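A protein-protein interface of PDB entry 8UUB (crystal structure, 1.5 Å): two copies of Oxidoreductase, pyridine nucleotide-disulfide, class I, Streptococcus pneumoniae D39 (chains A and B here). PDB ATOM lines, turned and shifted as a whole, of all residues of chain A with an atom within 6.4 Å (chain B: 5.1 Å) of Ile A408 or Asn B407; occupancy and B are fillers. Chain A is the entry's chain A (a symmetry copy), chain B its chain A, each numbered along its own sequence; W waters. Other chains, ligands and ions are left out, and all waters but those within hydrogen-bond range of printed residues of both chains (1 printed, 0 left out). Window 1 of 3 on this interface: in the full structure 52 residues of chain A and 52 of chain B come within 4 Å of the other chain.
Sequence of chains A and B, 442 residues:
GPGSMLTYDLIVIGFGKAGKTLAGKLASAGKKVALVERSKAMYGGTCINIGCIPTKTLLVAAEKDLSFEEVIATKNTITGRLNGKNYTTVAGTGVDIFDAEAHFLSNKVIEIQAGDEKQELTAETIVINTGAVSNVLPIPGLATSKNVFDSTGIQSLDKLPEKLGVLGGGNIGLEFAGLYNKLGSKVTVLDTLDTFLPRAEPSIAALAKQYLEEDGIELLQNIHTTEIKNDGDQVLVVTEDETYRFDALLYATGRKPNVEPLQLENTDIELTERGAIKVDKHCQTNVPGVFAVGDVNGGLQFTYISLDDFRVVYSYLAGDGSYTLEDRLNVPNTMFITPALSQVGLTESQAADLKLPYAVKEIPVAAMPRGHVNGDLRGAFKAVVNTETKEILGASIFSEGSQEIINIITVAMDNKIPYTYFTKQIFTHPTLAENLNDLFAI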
ATOM      1  N   GLU A 404      22.929  -0.333 -17.212  1.00  0.00           N
ATOM      2  CA  GLU A 404      22.769  -1.636 -16.572  1.00  0.00           C
ATOM      3  C   GLU A 404      21.657  -1.580 -15.520  1.00  0.00           C
ATOM      4  O   GLU A 404      20.799  -2.468 -15.495  1.00  0.00           O
ATOM      5  CB  GLU A 404      24.095  -2.012 -15.893  1.00  0.00           C
ATOM      6  CG  GLU A 404      25.330  -2.057 -16.846  1.00  0.00           C
ATOM      7  CD  GLU A 404      25.316  -3.045 -18.000  1.00  0.00           C
ATOM      8  OE1 GLU A 404      24.356  -3.803 -18.118  1.00  0.00           O
ATOM      9  OE2 GLU A 404      26.370  -3.107 -18.696  1.00  0.00           O
ATOM     10  N   ILE A 405      21.713  -0.555 -14.635  1.00  0.00           N
ATOM     11  CA  ILE A 405      20.820  -0.478 -13.466  1.00  0.00           C
ATOM     12  C   ILE A 405      19.340  -0.485 -13.887  1.00  0.00           C
ATOM     13  O   ILE A 405      18.507  -1.032 -13.165  1.00  0.00           O
ATOM     14  CB  ILE A 405      21.196   0.794 -12.682  1.00  0.00           C
ATOM     15  CG1 ILE A 405      22.605   0.688 -12.084  1.00  0.00           C
ATOM     16  CG2 ILE A 405      20.188   1.059 -11.550  1.00  0.00           C
ATOM     17  CD1 ILE A 405      23.126   2.018 -11.550  1.00  0.00           C
ATOM     18  N   ILE A 406      18.989   0.201 -14.977  1.00  0.00           N
ATOM     19  CA  ILE A 406      17.576   0.306 -15.363  1.00  0.00           C
ATOM     20  C   ILE A 406      16.937  -1.072 -15.495  1.00  0.00           C
ATOM     21  O   ILE A 406      15.759  -1.203 -15.253  1.00  0.00           O
ATOM     22  CB  ILE A 406      17.446   1.187 -16.609  1.00  0.00           C
ATOM     23  CG1 ILE A 406      16.006   1.616 -16.884  1.00  0.00           C
ATOM     24  CG2 ILE A 406      17.971   0.442 -17.862  1.00  0.00           C
ATOM     25  CD1 ILE A 406      15.468   2.603 -15.842  1.00  0.00           C
ATOM     26  N   ASN A 407      17.725  -2.066 -15.932  1.00  0.00           N
ATOM     27  CA  ASN A 407      17.140  -3.399 -16.115  1.00  0.00           C
ATOM     28  C   ASN A 407      16.702  -4.101 -14.823  1.00  0.00           C
ATOM     29  O   ASN A 407      15.934  -5.058 -14.865  1.00  0.00           O
ATOM     30  CB  ASN A 407      18.156  -4.262 -16.897  1.00  0.00           C
ATOM     31  CG  ASN A 407      18.565  -3.612 -18.206  1.00  0.00           C
ATOM     32  OD1 ASN A 407      17.726  -3.474 -19.124  1.00  0.00           O
ATOM     33  ND2 ASN A 407      19.823  -3.159 -18.322  1.00  0.00           N
ATOM     34  N   ILE A 408      17.233  -3.655 -13.660  1.00  0.00           N
ATOM     35  CA  ILE A 408      16.735  -4.116 -12.358  1.00  0.00           C
ATOM     36  C   ILE A 408      15.257  -3.776 -12.243  1.00  0.00           C
ATOM     37  O   ILE A 408      14.476  -4.614 -11.781  1.00  0.00           O
ATOM     38  CB  ILE A 408      17.543  -3.420 -11.236  1.00  0.00           C
ATOM     39  CG1 ILE A 408      19.010  -3.863 -11.315  1.00  0.00           C
ATOM     40  CG2 ILE A 408      16.923  -3.823  -9.870  1.00  0.00           C
ATOM     41  CD1 ILE A 408      19.890  -3.005 -10.374  1.00  0.00           C
ATOM     42  N   ILE A 409      14.908  -2.536 -12.638  1.00  0.00           N
ATOM     43  CA  ILE A 409      13.514  -2.074 -12.548  1.00  0.00           C
ATOM     44  C   ILE A 409      12.602  -2.950 -13.416  1.00  0.00           C
ATOM     45  O   ILE A 409      11.557  -3.411 -12.935  1.00  0.00           O
ATOM     46  CB  ILE A 409      13.373  -0.591 -12.953  1.00  0.00           C
ATOM     47  CG1 ILE A 409      14.329   0.321 -12.163  1.00  0.00           C
ATOM     48  CG2 ILE A 409      11.916  -0.126 -12.817  1.00  0.00           C
ATOM     49  CD1 ILE A 409      14.244   0.165 -10.623  1.00  0.00           C
ATOM     50  N   THR A 410      13.049  -3.193 -14.664  1.00  0.00           N
ATOM     51  CA  THR A 410      12.206  -3.942 -15.588  1.00  0.00           C
ATOM     52  C   THR A 410      11.846  -5.332 -15.034  1.00  0.00           C
ATOM     53  O   THR A 410      10.700  -5.784 -15.218  1.00  0.00           O
ATOM     54  CB  THR A 410      12.981  -4.115 -16.908  1.00  0.00           C
ATOM     55  OG1 THR A 410      13.372  -2.828 -17.346  1.00  0.00           O
ATOM     56  CG2 THR A 410      12.091  -4.759 -17.966  1.00  0.00           C
ATOM     57  N   VAL A 411      12.767  -6.026 -14.329  1.00  0.00           N
ATOM     58  CA  VAL A 411      12.461  -7.369 -13.845  1.00  0.00           C
ATOM     59  C   VAL A 411      11.235  -7.253 -12.922  1.00  0.00           C
ATOM     60  O   VAL A 411      10.297  -8.064 -12.981  1.00  0.00           O
ATOM     61  CB  VAL A 411      13.586  -7.926 -12.964  1.00  0.00           C
ATOM     62  CG1 VAL A 411      13.198  -9.311 -12.488  1.00  0.00           C
ATOM     63  CG2 VAL A 411      14.918  -8.055 -13.727  1.00  0.00           C
ATOM     64  N   ALA A 412      11.269  -6.253 -12.036  1.00  0.00           N
ATOM     65  CA  ALA A 412      10.160  -6.121 -11.081  1.00  0.00           C
ATOM     66  C   ALA A 412       8.872  -5.691 -11.794  1.00  0.00           C
ATOM     67  O   ALA A 412       7.789  -6.278 -11.506  1.00  0.00           O
ATOM     68  CB  ALA A 412      10.546  -5.097 -10.009  1.00  0.00           C
ATOM     69  N   MET A 413       8.918  -4.755 -12.746  1.00  0.00           N
ATOM     70  CA  MET A 413       7.702  -4.327 -13.455  1.00  0.00           C
ATOM     71  C   MET A 413       7.125  -5.515 -14.233  1.00  0.00           C
ATOM     72  O   MET A 413       5.918  -5.791 -14.148  1.00  0.00           O
ATOM     73  CB  MET A 413       7.957  -3.146 -14.392  1.00  0.00           C
ATOM     74  CG  MET A 413       8.367  -1.872 -13.645  1.00  0.00           C
ATOM     75  SD  MET A 413       8.795  -0.571 -14.822  1.00  0.00           S
ATOM     76  CE  MET A 413       7.181  -0.339 -15.575  1.00  0.00           C
ATOM     77  N   TYR A 421       9.205  -4.186  -2.511  1.00  0.00           N
ATOM     78  CA  TYR A 421      10.279  -5.176  -2.516  1.00  0.00           C
ATOM     79  C   TYR A 421      11.655  -4.487  -2.551  1.00  0.00           C
ATOM     80  O   TYR A 421      12.614  -4.965  -1.926  1.00  0.00           O
ATOM     81  CB  TYR A 421      10.128  -6.119  -3.750  1.00  0.00           C
ATOM     82  CG  TYR A 421      11.404  -6.881  -4.021  1.00  0.00           C
ATOM     83  CD1 TYR A 421      11.817  -7.931  -3.227  1.00  0.00           C
ATOM     84  CD2 TYR A 421      12.273  -6.473  -5.048  1.00  0.00           C
ATOM     85  CE1 TYR A 421      13.060  -8.560  -3.325  1.00  0.00           C
ATOM     86  CE2 TYR A 421      13.495  -7.097  -5.201  1.00  0.00           C
ATOM     87  CZ  TYR A 421      13.917  -8.098  -4.344  1.00  0.00           C
ATOM     88  OH  TYR A 421      15.115  -8.690  -4.530  1.00  0.00           O
ATOM     89  N   PHE A 422      11.710  -3.389  -3.274  1.00  0.00           N
ATOM     90  CA  PHE A 422      13.030  -2.766  -3.424  1.00  0.00           C
ATOM     91  C   PHE A 422      13.529  -2.158  -2.116  1.00  0.00           C
ATOM     92  O   PHE A 422      14.727  -1.908  -1.994  1.00  0.00           O
ATOM     93  CB  PHE A 422      13.073  -1.759  -4.577  1.00  0.00           C
ATOM     94  CG  PHE A 422      13.229  -2.405  -5.941  1.00  0.00           C
ATOM     95  CD1 PHE A 422      14.223  -3.325  -6.174  1.00  0.00           C
ATOM     96  CD2 PHE A 422      12.338  -2.069  -6.944  1.00  0.00           C
ATOM     97  CE1 PHE A 422      14.378  -3.887  -7.447  1.00  0.00           C
ATOM     98  CE2 PHE A 422      12.499  -2.630  -8.225  1.00  0.00           C
ATOM     99  CZ  PHE A 422      13.496  -3.578  -8.458  1.00  0.00           C
ATOM    100  N   GLN A 425      15.294  -5.545  -0.696  1.00  0.00           N
ATOM    101  CA  GLN A 425      16.360  -6.241  -1.415  1.00  0.00           C
ATOM    102  C   GLN A 425      17.714  -5.923  -0.757  1.00  0.00           C
ATOM    103  O   GLN A 425      17.997  -4.753  -0.360  1.00  0.00           O
ATOM    104  CB  GLN A 425      16.326  -5.772  -2.884  1.00  0.00           C
ATOM    105  CG  GLN A 425      17.495  -6.375  -3.698  1.00  0.00           C
ATOM    106  CD  GLN A 425      17.326  -6.227  -5.207  1.00  0.00           C
ATOM    107  OE1 GLN A 425      16.367  -5.615  -5.684  1.00  0.00           O
ATOM    108  NE2 GLN A 425      18.381  -6.699  -5.924  1.00  0.00           N
ATOM    109  N   ILE A 426      18.559  -6.941  -0.683  1.00  0.00           N
ATOM    110  CA  ILE A 426      19.920  -6.812  -0.170  1.00  0.00           C
ATOM    111  C   ILE A 426      20.835  -6.586  -1.396  1.00  0.00           C
ATOM    112  O   ILE A 426      21.097  -7.535  -2.165  1.00  0.00           O
ATOM    113  CB  ILE A 426      20.321  -8.049   0.668  1.00  0.00           C
ATOM    114  CG1 ILE A 426      19.325  -8.203   1.840  1.00  0.00           C
ATOM    115  CG2 ILE A 426      21.800  -7.943   1.130  1.00  0.00           C
ATOM    116  CD1 ILE A 426      19.549  -9.487   2.616  1.00  0.00           C
ATOM    117  N   PHE A 427      21.237  -5.322  -1.592  1.00  0.00           N
ATOM    118  CA  PHE A 427      22.089  -4.925  -2.725  1.00  0.00           C
ATOM    119  C   PHE A 427      23.552  -4.985  -2.353  1.00  0.00           C
ATOM    120  O   PHE A 427      23.919  -4.803  -1.193  1.00  0.00           O
ATOM    121  CB  PHE A 427      21.838  -3.455  -3.085  1.00  0.00           C
ATOM    122  CG  PHE A 427      20.526  -3.261  -3.795  1.00  0.00           C
ATOM    123  CD1 PHE A 427      20.438  -3.449  -5.180  1.00  0.00           C
ATOM    124  CD2 PHE A 427      19.374  -2.864  -3.117  1.00  0.00           C
ATOM    125  CE1 PHE A 427      19.233  -3.261  -5.864  1.00  0.00           C
ATOM    126  CE2 PHE A 427      18.170  -2.658  -3.820  1.00  0.00           C
ATOM    127  CZ  PHE A 427      18.104  -2.824  -5.207  1.00  0.00           C
ATOM    128  N   THR A 428      24.423  -5.174  -3.358  1.00  0.00           N
ATOM    129  CA  THR A 428      25.845  -4.972  -3.142  1.00  0.00           C
ATOM    130  C   THR A 428      26.090  -3.490  -2.803  1.00  0.00           C
ATOM    131  O   THR A 428      25.310  -2.598  -3.146  1.00  0.00           O
ATOM    132  CB  THR A 428      26.681  -5.368  -4.368  1.00  0.00           C
ATOM    133  OG1 THR A 428      25.971  -4.815  -5.509  1.00  0.00           O
ATOM    134  CG2 THR A 428      26.720  -6.875  -4.521  1.00  0.00           C
ATOM    135  N   THR A 431      27.465   0.790  -4.257  1.00  0.00           N
ATOM    136  CA  THR A 431      26.983   0.777  -5.654  1.00  0.00           C
ATOM    137  C   THR A 431      25.978   1.908  -5.818  1.00  0.00           C
ATOM    138  O   THR A 431      25.542   2.537  -4.850  1.00  0.00           O
ATOM    139  CB  THR A 431      26.276  -0.549  -6.032  1.00  0.00           C
ATOM    140  OG1 THR A 431      25.098  -0.673  -5.196  1.00  0.00           O
ATOM    141  CG2 THR A 431      27.179  -1.737  -5.805  1.00  0.00           C
ATOM    142  N   ALA A 433      23.106   1.096  -7.515  1.00  0.00           N
ATOM    143  CA  ALA A 433      21.860   0.354  -7.382  1.00  0.00           C
ATOM    144  C   ALA A 433      21.325   0.257  -5.950  1.00  0.00           C
ATOM    145  O   ALA A 433      20.094   0.255  -5.798  1.00  0.00           O
ATOM    146  CB  ALA A 433      21.991  -1.044  -7.977  1.00  0.00           C
ATOM    147  N   GLU A 434      22.171   0.257  -4.920  1.00  0.00           N
ATOM    148  CA  GLU A 434      21.593   0.070  -3.597  1.00  0.00           C
ATOM    149  C   GLU A 434      20.690   1.245  -3.222  1.00  0.00           C
ATOM    150  O   GLU A 434      19.828   1.149  -2.340  1.00  0.00           O
ATOM    151  CB  GLU A 434      22.699  -0.089  -2.565  1.00  0.00           C
ATOM    152  CG  GLU A 434      23.579   1.151  -2.479  1.00  0.00           C
ATOM    153  CD  GLU A 434      24.732   0.872  -1.555  1.00  0.00           C
ATOM    154  OE1 GLU A 434      24.461   0.290  -0.478  1.00  0.00           O
ATOM    155  OE2 GLU A 434      25.888   1.257  -1.900  1.00  0.00           O
ATOM    156  N   LEU A 436      18.273   2.203  -4.656  1.00  0.00           N
ATOM    157  CA  LEU A 436      16.884   1.807  -4.856  1.00  0.00           C
ATOM    158  C   LEU A 436      16.212   1.439  -3.515  1.00  0.00           C
ATOM    159  O   LEU A 436      14.988   1.561  -3.403  1.00  0.00           O
ATOM    160  CB  LEU A 436      16.791   0.622  -5.837  1.00  0.00           C
ATOM    161  CG  LEU A 436      17.315   0.974  -7.240  1.00  0.00           C
ATOM    162  CD1 LEU A 436      17.208  -0.303  -8.103  1.00  0.00           C
ATOM    163  CD2 LEU A 436      16.561   2.148  -7.866  1.00  0.00           C
ATOM    164  N   PRO B 332      24.100 -11.066  -2.261  1.00  0.00           N
ATOM    165  CA  PRO B 332      25.165 -11.079  -3.274  1.00  0.00           C
ATOM    166  C   PRO B 332      26.483 -10.639  -2.659  1.00  0.00           C
ATOM    167  O   PRO B 332      26.528 -10.205  -1.497  1.00  0.00           O
ATOM    168  CB  PRO B 332      24.666  -9.974  -4.241  1.00  0.00           C
ATOM    169  CG  PRO B 332      24.001  -8.926  -3.298  1.00  0.00           C
ATOM    170  CD  PRO B 332      23.305  -9.831  -2.248  1.00  0.00           C
ATOM    171  N   SER B 402      29.795  -5.195 -12.995  1.00  0.00           N
ATOM    172  CA  SER B 402      29.113  -6.359 -12.424  1.00  0.00           C
ATOM    173  C   SER B 402      28.496  -6.082 -11.045  1.00  0.00           C
ATOM    174  O   SER B 402      27.513  -6.734 -10.688  1.00  0.00           O
ATOM    175  CB  SER B 402      30.029  -7.554 -12.288  1.00  0.00           C
ATOM    176  OG  SER B 402      31.004  -7.315 -11.246  1.00  0.00           O
ATOM    177  N   GLN B 403      29.070  -5.103 -10.308  1.00  0.00           N
ATOM    178  CA  GLN B 403      28.527  -4.804  -8.994  1.00  0.00           C
ATOM    179  C   GLN B 403      27.116  -4.238  -9.125  1.00  0.00           C
ATOM    180  O   GLN B 403      26.323  -4.333  -8.153  1.00  0.00           O
ATOM    181  CB  GLN B 403      29.453  -3.800  -8.247  1.00  0.00           C
ATOM    182  CG  GLN B 403      29.418  -2.333  -8.731  1.00  0.00           C
ATOM    183  CD  GLN B 403      30.277  -2.072  -9.946  1.00  0.00           C
ATOM    184  OE1 GLN B 403      30.832  -2.955 -10.605  1.00  0.00           O
ATOM    185  NE2 GLN B 403      30.412  -0.798 -10.279  1.00  0.00           N
ATOM    186  N   GLU B 404      26.736  -3.625 -10.273  1.00  0.00           N
ATOM    187  CA  GLU B 404      25.342  -3.253 -10.502  1.00  0.00           C
ATOM    188  C   GLU B 404      24.556  -4.447 -11.053  1.00  0.00           C
ATOM    189  O   GLU B 404      23.459  -4.731 -10.561  1.00  0.00           O
ATOM    190  CB  GLU B 404      25.305  -2.105 -11.521  1.00  0.00           C
ATOM    191  CG  GLU B 404      26.113  -0.835 -11.108  1.00  0.00           C
ATOM    192  CD  GLU B 404      25.706  -0.100  -9.843  1.00  0.00           C
ATOM    193  OE1 GLU B 404      24.730  -0.502  -9.214  1.00  0.00           O
ATOM    194  OE2 GLU B 404      26.332   0.969  -9.591  1.00  0.00           O
ATOM    195  N   ILE B 405      25.111  -5.107 -12.099  1.00  0.00           N
ATOM    196  CA  ILE B 405      24.386  -6.153 -12.840  1.00  0.00           C
ATOM    197  C   ILE B 405      23.945  -7.297 -11.913  1.00  0.00           C
ATOM    198  O   ILE B 405      22.886  -7.884 -12.134  1.00  0.00           O
ATOM    199  CB  ILE B 405      25.314  -6.643 -13.969  1.00  0.00           C
ATOM    200  CG1 ILE B 405      25.567  -5.541 -15.006  1.00  0.00           C
ATOM    201  CG2 ILE B 405      24.715  -7.872 -14.676  1.00  0.00           C
ATOM    202  CD1 ILE B 405      26.693  -5.884 -15.975  1.00  0.00           C
ATOM    203  N   ILE B 406      24.783  -7.691 -10.951  1.00  0.00           N
ATOM    204  CA  ILE B 406      24.449  -8.843 -10.103  1.00  0.00           C
ATOM    205  C   ILE B 406      23.087  -8.665  -9.443  1.00  0.00           C
ATOM    206  O   ILE B 406      22.417  -9.642  -9.196  1.00  0.00           O
ATOM    207  CB  ILE B 406      25.597  -9.114  -9.126  1.00  0.00           C
ATOM    208  CG1 ILE B 406      25.483 -10.474  -8.440  1.00  0.00           C
ATOM    209  CG2 ILE B 406      25.645  -8.026  -8.024  1.00  0.00           C
ATOM    210  CD1 ILE B 406      25.711 -11.647  -9.401  1.00  0.00           C
ATOM    211  N   ASN B 407      22.729  -7.413  -9.119  1.00  0.00           N
ATOM    212  CA  ASN B 407      21.445  -7.200  -8.442  1.00  0.00           C
ATOM    213  C   ASN B 407      20.204  -7.505  -9.291  1.00  0.00           C
ATOM    214  O   ASN B 407      19.110  -7.664  -8.757  1.00  0.00           O
ATOM    215  CB  ASN B 407      21.416  -5.746  -7.921  1.00  0.00           C
ATOM    216  CG  ASN B 407      22.609  -5.436  -7.035  1.00  0.00           C
ATOM    217  OD1 ASN B 407      22.729  -6.004  -5.927  1.00  0.00           O
ATOM    218  ND2 ASN B 407      23.535  -4.579  -7.496  1.00  0.00           N
ATOM    219  N   ILE B 408      20.360  -7.539 -10.635  1.00  0.00           N
ATOM    220  CA  ILE B 408      19.292  -8.016 -11.524  1.00  0.00           C
ATOM    221  C   ILE B 408      18.945  -9.451 -11.156  1.00  0.00           C
ATOM    222  O   ILE B 408      17.759  -9.792 -11.099  1.00  0.00           O
ATOM    223  CB  ILE B 408      19.785  -7.933 -12.990  1.00  0.00           C
ATOM    224  CG1 ILE B 408      20.029  -6.464 -13.363  1.00  0.00           C
ATOM    225  CG2 ILE B 408      18.694  -8.555 -13.903  1.00  0.00           C
ATOM    226  CD1 ILE B 408      20.752  -6.361 -14.727  1.00  0.00           C
ATOM    227  N   ILE B 409      19.992 -10.272 -10.946  1.00  0.00           N
ATOM    228  CA  ILE B 409      19.790 -11.691 -10.614  1.00  0.00           C
ATOM    229  C   ILE B 409      19.011 -11.828  -9.299  1.00  0.00           C
ATOM    230  O   ILE B 409      18.029 -12.582  -9.244  1.00  0.00           O
ATOM    231  CB  ILE B 409      21.127 -12.457 -10.525  1.00  0.00           C
ATOM    232  CG1 ILE B 409      21.982 -12.283 -11.793  1.00  0.00           C
ATOM    233  CG2 ILE B 409      20.884 -13.941 -10.212  1.00  0.00           C
ATOM    234  CD1 ILE B 409      21.247 -12.618 -13.117  1.00  0.00           C
ATOM    235  N   THR B 410      19.447 -11.055  -8.285  1.00  0.00           N
ATOM    236  CA  THR B 410      18.824 -11.186  -6.973  1.00  0.00           C
ATOM    237  C   THR B 410      17.309 -10.919  -7.032  1.00  0.00           C
ATOM    238  O   THR B 410      16.540 -11.616  -6.342  1.00  0.00           O
ATOM    239  CB  THR B 410      19.476 -10.157  -6.030  1.00  0.00           C
ATOM    240  OG1 THR B 410      20.874 -10.372  -6.065  1.00  0.00           O
ATOM    241  CG2 THR B 410      18.971 -10.349  -4.603  1.00  0.00           C
ATOM    242  N   VAL B 411      16.834  -9.958  -7.855  1.00  0.00           N
ATOM    243  CA  VAL B 411      15.406  -9.654  -7.881  1.00  0.00           C
ATOM    244  C   VAL B 411      14.673 -10.945  -8.286  1.00  0.00           C
ATOM    245  O   VAL B 411      13.640 -11.315  -7.706  1.00  0.00           O
ATOM    246  CB  VAL B 411      15.063  -8.628  -8.968  1.00  0.00           C
ATOM    247  CG1 VAL B 411      13.571  -8.371  -8.948  1.00  0.00           C
ATOM    248  CG2 VAL B 411      15.769  -7.278  -8.744  1.00  0.00           C
HETATM  249  O   HOH W   1      20.996  -7.772  -4.886  1.00  0.00           O
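Of the 20 printed residues of chain A, 13 touch a printed residue of chain B.
Hydrophobic or aromatic side chains of chain A within 4 Å of the printed part of chain B: Ile A405, Ile A408, Val A411, Tyr A421, Phe A422, Phe A427 and Ala A433.
Among the printed residues, no Asp or Glu carboxylate lies within 4 Å of a Lys or Arg side-chain nitrogen of the other chain.
Glu A404 touches Ile B408, and with the chains exchanged Ile A408 touches Glu B404.
Asn A407 touches Ile B408, and with the chains exchanged Ile A408 touches Asn B407.
Ile A408 touches Val B411, and with the chains exchanged Val A411 touches Ile B408.
Val A411 touches its own counterpart, Val B411.
Positions printed for both chains: 404, 405, 406, 407, 408, 409, 410 and 411.
Of the 26 pairs that touch across the chains among the printed residues, 10 have their exchanged pair printed and touching as well.
Water W1 lies within hydrogen-bond range of OD1 of Asn B407, O of Ile A426, OG1 of Thr B410 and NE2 of Gln A425.
The backbone carbonyl oxygen (O) of Glu A404 sits at hydrogen-bond distance from the side-chain amide nitrogen (ND2) of Asn A407 (3.1 Å).
The side-chain hydroxyl (OG1) of Thr A431 lies within hydrogen-bond range of the backbone carbonyl oxygen (O) of Thr A428 (2.8 Å).
ND2 of Asn B407 lies within hydrogen-bond range of O of Gln B403, at 2.9 Å.
O of Glu B404 is in hydrogen-bond range of ND2 of Asn B407 (3.1 Å).
N of Thr A431 lies within hydrogen-bond range of OE2 of Glu A434 (2.9 Å).
The backbone carbonyl oxygen of Asn B407 lies within hydrogen-bond range of the side-chain amide nitrogen of Gln A425.
ND2 of Asn B407 is in hydrogen-bond range of OG1 of Thr A428 (3.2 Å).
N of Ala A433 lies within hydrogen-bond range of OE1 of Glu B404.
OG1 of Thr A428 lies within hydrogen-bond range of O of Gln B403.
Among the printed residues, pairs that only touch across the chains: Ile A426 with Pro B332, Phe A427 with Asn B407, Ile A408 with Ile B408, Tyr A421 with Val B411, Gln A425 with Val B411, Thr A431 with Glu B404, Thr A431 with Gln B403, Thr A428 with Pro B332, Gln A425 with Thr B410, Val A411 with Val B411, Tyr A421 with Thr B410, Ile A405 with Glu B404, Glu A404 with Ile B405, Ile A408 with Val B411, Val A411 with Ile B408, Thr A428 with Ile B406, Ala A433 with Asn B407, Phe A422 with Val B411, Glu A404 with Ile B408, Ile A408 with Glu B404, Asn A407 with Ile B408 and Ile A408 with Asn B407.
Printed residues of chain B within 4 Å of Ile A408: Glu B404, Asn B407, Ile B408 and Val B411.
Of the printed residues of chain B, Val A411 touches Ile B408 and Val B411.
Of the printed residues of chain B, Tyr A421 touches Thr B410 and Val B411.
Leu A436 touches none of the printed residues of chain B.
Of the printed residues of chain A, Asn B407 touches Ile A408 (3.98 Å), Gln A425 (3.1 Å), Phe A427 (3.4 Å), Thr A428 (3.2 Å) and Ala A433 (3.9 Å).
The nearest printed residue of chain A that does not touch Ile B405 is Ile A408 (5.6 Å).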
